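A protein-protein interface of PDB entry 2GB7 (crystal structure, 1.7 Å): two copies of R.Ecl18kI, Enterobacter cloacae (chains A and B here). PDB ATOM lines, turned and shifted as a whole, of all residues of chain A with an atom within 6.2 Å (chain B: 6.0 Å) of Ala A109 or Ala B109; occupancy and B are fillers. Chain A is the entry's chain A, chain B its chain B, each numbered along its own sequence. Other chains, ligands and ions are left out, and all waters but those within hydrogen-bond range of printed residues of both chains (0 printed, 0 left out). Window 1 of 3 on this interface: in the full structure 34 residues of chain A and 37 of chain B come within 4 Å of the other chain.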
ATOM      1  N   HIS A 104     -12.349 -17.387  -8.228  1.00  0.00           N
ATOM      2  CA  HIS A 104     -13.571 -17.556  -7.412  1.00  0.00           C
ATOM      3  C   HIS A 104     -13.713 -19.011  -6.984  1.00  0.00           C
ATOM      4  O   HIS A 104     -13.844 -19.314  -5.768  1.00  0.00           O
ATOM      5  CB  HIS A 104     -14.803 -17.144  -8.209  1.00  0.00           C
ATOM      6  CG  HIS A 104     -14.753 -15.754  -8.758  1.00  0.00           C
ATOM      7  ND1 HIS A 104     -13.857 -15.370  -9.736  1.00  0.00           N
ATOM      8  CD2 HIS A 104     -15.527 -14.670  -8.502  1.00  0.00           C
ATOM      9  CE1 HIS A 104     -14.067 -14.104 -10.043  1.00  0.00           C
ATOM     10  NE2 HIS A 104     -15.082 -13.657  -9.316  1.00  0.00           N
ATOM     11  N   ILE A 105     -13.610 -19.907  -7.977  1.00  0.00           N
ATOM     12  CA  ILE A 105     -13.624 -21.368  -7.725  1.00  0.00           C
ATOM     13  C   ILE A 105     -12.520 -21.825  -6.775  1.00  0.00           C
ATOM     14  O   ILE A 105     -12.755 -22.490  -5.742  1.00  0.00           O
ATOM     15  CB  ILE A 105     -13.535 -22.164  -9.056  1.00  0.00           C
ATOM     16  CG1 ILE A 105     -14.678 -21.784 -10.010  1.00  0.00           C
ATOM     17  CG2 ILE A 105     -13.522 -23.660  -8.788  1.00  0.00           C
ATOM     18  CD1 ILE A 105     -14.601 -22.455 -11.379  1.00  0.00           C
ATOM     19  N   TYR A 106     -11.287 -21.468  -7.093  1.00  0.00           N
ATOM     20  CA  TYR A 106     -10.205 -21.691  -6.142  1.00  0.00           C
ATOM     21  C   TYR A 106     -10.520 -21.138  -4.736  1.00  0.00           C
ATOM     22  O   TYR A 106     -10.306 -21.816  -3.716  1.00  0.00           O
ATOM     23  CB  TYR A 106      -8.889 -21.097  -6.666  1.00  0.00           C
ATOM     24  CG  TYR A 106      -7.768 -21.180  -5.656  1.00  0.00           C
ATOM     25  CD1 TYR A 106      -7.138 -22.394  -5.399  1.00  0.00           C
ATOM     26  CD2 TYR A 106      -7.324 -20.044  -4.922  1.00  0.00           C
ATOM     27  CE1 TYR A 106      -6.125 -22.501  -4.453  1.00  0.00           C
ATOM     28  CE2 TYR A 106      -6.279 -20.126  -3.963  1.00  0.00           C
ATOM     29  CZ  TYR A 106      -5.660 -21.342  -3.734  1.00  0.00           C
ATOM     30  OH  TYR A 106      -4.666 -21.373  -2.809  1.00  0.00           O
ATOM     31  N   ASP A 107     -11.065 -19.922  -4.676  1.00  0.00           N
ATOM     32  CA  ASP A 107     -11.294 -19.275  -3.371  1.00  0.00           C
ATOM     33  C   ASP A 107     -12.355 -19.992  -2.524  1.00  0.00           C
ATOM     34  O   ASP A 107     -12.186 -20.106  -1.299  1.00  0.00           O
ATOM     35  CB  ASP A 107     -11.648 -17.806  -3.548  1.00  0.00           C
ATOM     36  CG  ASP A 107     -10.447 -16.974  -3.988  1.00  0.00           C
ATOM     37  OD1 ASP A 107      -9.312 -17.455  -3.882  1.00  0.00           O
ATOM     38  OD2 ASP A 107     -10.655 -15.848  -4.492  1.00  0.00           O
ATOM     39  N   LEU A 108     -13.417 -20.458  -3.178  1.00  0.00           N
ATOM     40  CA  LEU A 108     -14.418 -21.323  -2.532  1.00  0.00           C
ATOM     41  C   LEU A 108     -13.754 -22.583  -1.942  1.00  0.00           C
ATOM     42  O   LEU A 108     -13.923 -22.893  -0.744  1.00  0.00           O
ATOM     43  CB  LEU A 108     -15.500 -21.719  -3.531  1.00  0.00           C
ATOM     44  CG  LEU A 108     -16.489 -22.791  -3.038  1.00  0.00           C
ATOM     45  CD1 LEU A 108     -17.134 -22.401  -1.706  1.00  0.00           C
ATOM     46  CD2 LEU A 108     -17.527 -22.925  -4.128  1.00  0.00           C
ATOM     47  N   ALA A 109     -13.024 -23.316  -2.792  1.00  0.00           N
ATOM     48  CA  ALA A 109     -12.332 -24.544  -2.324  1.00  0.00           C
ATOM     49  C   ALA A 109     -11.310 -24.291  -1.240  1.00  0.00           C
ATOM     50  O   ALA A 109     -11.144 -25.126  -0.317  1.00  0.00           O
ATOM     51  CB  ALA A 109     -11.671 -25.261  -3.490  1.00  0.00           C
ATOM     52  N   LEU A 110     -10.555 -23.180  -1.354  1.00  0.00           N
ATOM     53  CA  LEU A 110      -9.601 -22.765  -0.310  1.00  0.00           C
ATOM     54  C   LEU A 110     -10.346 -22.560   1.014  1.00  0.00           C
ATOM     55  O   LEU A 110      -9.932 -23.085   2.053  1.00  0.00           O
ATOM     56  CB  LEU A 110      -8.893 -21.468  -0.727  1.00  0.00           C
ATOM     57  CG  LEU A 110      -7.987 -20.887   0.351  1.00  0.00           C
ATOM     58  CD1 LEU A 110      -6.915 -21.900   0.734  1.00  0.00           C
ATOM     59  CD2 LEU A 110      -7.386 -19.593  -0.193  1.00  0.00           C
ATOM     60  N   SER A 111     -11.473 -21.834   0.960  1.00  0.00           N
ATOM     61  CA  SER A 111     -12.286 -21.606   2.158  1.00  0.00           C
ATOM     62  C   SER A 111     -12.707 -22.960   2.749  1.00  0.00           C
ATOM     63  O   SER A 111     -12.622 -23.176   3.974  1.00  0.00           O
ATOM     64  CB  SER A 111     -13.481 -20.703   1.838  1.00  0.00           C
ATOM     65  OG  SER A 111     -14.203 -20.366   3.015  1.00  0.00           O
ATOM     66  N   ASN A 112     -13.035 -23.907   1.875  1.00  0.00           N
ATOM     67  CA  ASN A 112     -13.501 -25.239   2.312  1.00  0.00           C
ATOM     68  C   ASN A 112     -12.388 -26.020   3.001  1.00  0.00           C
ATOM     69  O   ASN A 112     -12.592 -26.602   4.079  1.00  0.00           O
ATOM     70  CB  ASN A 112     -14.063 -26.049   1.133  1.00  0.00           C
ATOM     71  CG  ASN A 112     -15.451 -25.612   0.701  1.00  0.00           C
ATOM     72  OD1 ASN A 112     -16.119 -24.780   1.344  1.00  0.00           O
ATOM     73  ND2 ASN A 112     -15.927 -26.225  -0.384  1.00  0.00           N
ATOM     74  N   THR A 113     -11.217 -26.089   2.383  1.00  0.00           N
ATOM     75  CA  THR A 113     -10.114 -26.764   3.066  1.00  0.00           C
ATOM     76  C   THR A 113      -9.751 -26.138   4.415  1.00  0.00           C
ATOM     77  O   THR A 113      -9.417 -26.853   5.373  1.00  0.00           O
ATOM     78  CB  THR A 113      -8.850 -27.062   2.166  1.00  0.00           C
ATOM     79  OG1 THR A 113      -7.989 -27.943   2.874  1.00  0.00           O
ATOM     80  CG2 THR A 113      -8.044 -25.833   1.774  1.00  0.00           C
ATOM     81  N   GLN A 114      -9.767 -24.805   4.492  1.00  0.00           N
ATOM     82  CA  GLN A 114      -9.421 -24.103   5.721  1.00  0.00           C
ATOM     83  C   GLN A 114     -10.444 -24.401   6.832  1.00  0.00           C
ATOM     84  O   GLN A 114     -10.063 -24.591   8.024  1.00  0.00           O
ATOM     85  CB  GLN A 114      -9.291 -22.596   5.468  1.00  0.00           C
ATOM     86  CG  GLN A 114      -8.173 -22.217   4.464  1.00  0.00           C
ATOM     87  CD  GLN A 114      -6.771 -22.329   5.035  1.00  0.00           C
ATOM     88  OE1 GLN A 114      -6.264 -23.427   5.311  1.00  0.00           O
ATOM     89  NE2 GLN A 114      -6.133 -21.183   5.243  1.00  0.00           N
ATOM     90  N   HIS B 104     -13.429 -33.491  -7.761  1.00  0.00           N
ATOM     91  CA  HIS B 104     -12.422 -33.138  -8.759  1.00  0.00           C
ATOM     92  C   HIS B 104     -11.959 -31.690  -8.627  1.00  0.00           C
ATOM     93  O   HIS B 104     -10.757 -31.423  -8.517  1.00  0.00           O
ATOM     94  CB  HIS B 104     -12.983 -33.346 -10.172  1.00  0.00           C
ATOM     95  CG  HIS B 104     -13.351 -34.762 -10.476  1.00  0.00           C
ATOM     96  ND1 HIS B 104     -14.570 -35.300 -10.126  1.00  0.00           N
ATOM     97  CD2 HIS B 104     -12.675 -35.741 -11.123  1.00  0.00           C
ATOM     98  CE1 HIS B 104     -14.635 -36.550 -10.554  1.00  0.00           C
ATOM     99  NE2 HIS B 104     -13.494 -36.845 -11.154  1.00  0.00           N
ATOM    100  N   ILE B 105     -12.918 -30.766  -8.654  1.00  0.00           N
ATOM    101  CA  ILE B 105     -12.645 -29.329  -8.608  1.00  0.00           C
ATOM    102  C   ILE B 105     -11.975 -29.002  -7.286  1.00  0.00           C
ATOM    103  O   ILE B 105     -10.952 -28.295  -7.242  1.00  0.00           O
ATOM    104  CB  ILE B 105     -13.949 -28.516  -8.773  1.00  0.00           C
ATOM    105  CG1 ILE B 105     -14.505 -28.735 -10.176  1.00  0.00           C
ATOM    106  CG2 ILE B 105     -13.702 -27.017  -8.576  1.00  0.00           C
ATOM    107  CD1 ILE B 105     -15.865 -28.073 -10.407  1.00  0.00           C
ATOM    108  N   TYR B 106     -12.522 -29.549  -6.209  1.00  0.00           N
ATOM    109  CA  TYR B 106     -11.926 -29.362  -4.885  1.00  0.00           C
ATOM    110  C   TYR B 106     -10.501 -29.916  -4.840  1.00  0.00           C
ATOM    111  O   TYR B 106      -9.609 -29.248  -4.326  1.00  0.00           O
ATOM    112  CB  TYR B 106     -12.801 -29.982  -3.784  1.00  0.00           C
ATOM    113  CG  TYR B 106     -12.110 -29.928  -2.430  1.00  0.00           C
ATOM    114  CD1 TYR B 106     -12.085 -28.769  -1.673  1.00  0.00           C
ATOM    115  CD2 TYR B 106     -11.477 -31.061  -1.922  1.00  0.00           C
ATOM    116  CE1 TYR B 106     -11.419 -28.724  -0.429  1.00  0.00           C
ATOM    117  CE2 TYR B 106     -10.820 -31.030  -0.689  1.00  0.00           C
ATOM    118  CZ  TYR B 106     -10.801 -29.862   0.051  1.00  0.00           C
ATOM    119  OH  TYR B 106     -10.164 -29.831   1.276  1.00  0.00           O
ATOM    120  N   ASP B 107     -10.276 -31.125  -5.353  1.00  0.00           N
ATOM    121  CA  ASP B 107      -8.938 -31.725  -5.354  1.00  0.00           C
ATOM    122  C   ASP B 107      -7.900 -30.905  -6.117  1.00  0.00           C
ATOM    123  O   ASP B 107      -6.731 -30.788  -5.697  1.00  0.00           O
ATOM    124  CB  ASP B 107      -8.987 -33.125  -5.933  1.00  0.00           C
ATOM    125  CG  ASP B 107      -9.624 -34.116  -4.984  1.00  0.00           C
ATOM    126  OD1 ASP B 107      -9.868 -33.755  -3.804  1.00  0.00           O
ATOM    127  OD2 ASP B 107      -9.867 -35.255  -5.436  1.00  0.00           O
ATOM    128  N   LEU B 108      -8.319 -30.358  -7.252  1.00  0.00           N
ATOM    129  CA  LEU B 108      -7.444 -29.429  -7.979  1.00  0.00           C
ATOM    130  C   LEU B 108      -7.091 -28.197  -7.157  1.00  0.00           C
ATOM    131  O   LEU B 108      -5.919 -27.827  -7.066  1.00  0.00           O
ATOM    132  CB  LEU B 108      -8.101 -28.992  -9.288  1.00  0.00           C
ATOM    133  CG  LEU B 108      -7.391 -27.933 -10.136  1.00  0.00           C
ATOM    134  CD1 LEU B 108      -6.016 -28.392 -10.572  1.00  0.00           C
ATOM    135  CD2 LEU B 108      -8.222 -27.590 -11.372  1.00  0.00           C
ATOM    136  N   ALA B 109      -8.097 -27.527  -6.597  1.00  0.00           N
ATOM    137  CA  ALA B 109      -7.820 -26.328  -5.805  1.00  0.00           C
ATOM    138  C   ALA B 109      -6.974 -26.669  -4.591  1.00  0.00           C
ATOM    139  O   ALA B 109      -6.054 -25.927  -4.247  1.00  0.00           O
ATOM    140  CB  ALA B 109      -9.106 -25.671  -5.370  1.00  0.00           C
ATOM    141  N   LEU B 110      -7.286 -27.796  -3.959  1.00  0.00           N
ATOM    142  CA  LEU B 110      -6.497 -28.253  -2.820  1.00  0.00           C
ATOM    143  C   LEU B 110      -5.023 -28.425  -3.197  1.00  0.00           C
ATOM    144  O   LEU B 110      -4.141 -27.924  -2.490  1.00  0.00           O
ATOM    145  CB  LEU B 110      -7.036 -29.563  -2.232  1.00  0.00           C
ATOM    146  CG  LEU B 110      -6.282 -30.189  -1.043  1.00  0.00           C
ATOM    147  CD1 LEU B 110      -6.200 -29.242   0.158  1.00  0.00           C
ATOM    148  CD2 LEU B 110      -6.992 -31.509  -0.670  1.00  0.00           C
ATOM    149  N   SER B 111      -4.777 -29.122  -4.307  1.00  0.00           N
ATOM    150  CA  SER B 111      -3.422 -29.351  -4.807  1.00  0.00           C
ATOM    151  C   SER B 111      -2.716 -28.010  -5.042  1.00  0.00           C
ATOM    152  O   SER B 111      -1.546 -27.847  -4.653  1.00  0.00           O
ATOM    153  CB  SER B 111      -3.490 -30.160  -6.107  1.00  0.00           C
ATOM    154  OG  SER B 111      -2.198 -30.517  -6.556  1.00  0.00           O
ATOM    155  N   ASN B 112      -3.435 -27.067  -5.660  1.00  0.00           N
ATOM    156  CA  ASN B 112      -2.946 -25.676  -5.850  1.00  0.00           C
ATOM    157  C   ASN B 112      -2.536 -24.952  -4.575  1.00  0.00           C
ATOM    158  O   ASN B 112      -1.443 -24.353  -4.523  1.00  0.00           O
ATOM    159  CB  ASN B 112      -3.988 -24.821  -6.567  1.00  0.00           C
ATOM    160  CG  ASN B 112      -4.072 -25.118  -8.052  1.00  0.00           C
ATOM    161  OD1 ASN B 112      -3.292 -25.897  -8.610  1.00  0.00           O
ATOM    162  ND2 ASN B 112      -5.021 -24.470  -8.702  1.00  0.00           N
ATOM    163  N   THR B 113      -3.388 -24.982  -3.540  1.00  0.00           N
ATOM    164  CA  THR B 113      -2.997 -24.276  -2.310  1.00  0.00           C
ATOM    165  C   THR B 113      -1.861 -24.978  -1.590  1.00  0.00           C
ATOM    166  O   THR B 113      -1.014 -24.323  -0.945  1.00  0.00           O
ATOM    167  CB  THR B 113      -4.161 -23.992  -1.314  1.00  0.00           C
ATOM    168  OG1 THR B 113      -3.688 -23.130  -0.260  1.00  0.00           O
ATOM    169  CG2 THR B 113      -4.799 -25.296  -0.761  1.00  0.00           C
ATOM    170  N   GLN B 114      -1.818 -26.302  -1.695  1.00  0.00           N
ATOM    171  CA  GLN B 114      -0.697 -27.025  -1.045  1.00  0.00           C
ATOM    172  C   GLN B 114       0.631 -26.750  -1.741  1.00  0.00           C
ATOM    173  O   GLN B 114       1.705 -26.622  -1.089  1.00  0.00           O
ATOM    174  CB  GLN B 114      -0.981 -28.516  -0.999  1.00  0.00           C
ATOM    175  CG  GLN B 114      -2.239 -28.872  -0.216  1.00  0.00           C
ATOM    176  CD  GLN B 114      -2.051 -28.701   1.295  1.00  0.00           C
ATOM    177  OE1 GLN B 114      -1.887 -27.581   1.809  1.00  0.00           O
ATOM    178  NE2 GLN B 114      -2.031 -29.820   2.007  1.00  0.00           N
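The side-chain hydroxyl (OG1) of Thr A113 lies close to the side-chain hydroxyl (OH) of Tyr B106, at 3.3 Å. OH of Tyr A106 sits close to OG1 of Thr B113 (3.2 Å).
Among the printed residues, merely in contact across the chains: Ile A105 with Ile B105 (3.4 Å), Tyr A106 with Ala B109 (3.4 Å), Tyr A106 with Asn B112 (3.8 Å), Ala A109 with Tyr B106 (3.6 Å), Ala A109 with Ala B109 (3.2 Å), Leu A110 with Thr B113 (3.6 Å) and Thr A113 with Leu B110 (3.5 Å).
Ala A109 touches two residues of chain B. Of chain A, only Tyr A106 (3.4 Å) and Ala A109 (3.2 Å) come within 4 Å of Ala B109. Of the printed residues of chain B, Thr A113 touches Tyr B106 (3.2 Å) and Leu B110 (3.5 Å). Printed residues of chain A within 4 Å of Ile B105: Ile A105 (3.4 Å). Of the printed residues of chain A, Tyr B106 touches Ala A109 (3.6 Å) and Thr A113 (3.2 Å). Printed residues of chain B within 4 Å of Leu A110: Thr B113 (3.6 Å). Printed residues of chain B within 4 Å of Tyr A106: Ala B109, Asn B112 and Thr B113. The nearest residue of chain B that does not touch Ala A109 is Ile B105 (4.9 Å). The nearest residue of chain A that does not touch Ala B109 is Ile A105 (4.9 Å).
Of the 11 printed residues of chain B, 6 touch a printed residue of chain A. Hydrophobic or aromatic side chains of chain A within 4 Å of the printed part of chain B: Ile A105, Tyr A106, Ala A109 and Leu A110. Along chain A the printed residues that touch a printed residue of chain B span positions 105 to 113. Among the printed residues, 9 pairs touch across the chains.
Tyr A106 touches Ala B109, and with the chains exchanged Ala A109 touches Tyr B106. Tyr A106 touches Asn B112, but with the chains exchanged Asn A112 does not touch Tyr B106 (4.1 Å). Ala A109 touches its own counterpart, Ala B109. Leu A110 touches Thr B113, and with the chains exchanged Thr A113 touches Leu B110. 11 positions are printed for both chains. Of the 9 pairs that touch across the chains among the printed residues, 8 have their exchanged pair printed and touching as well.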
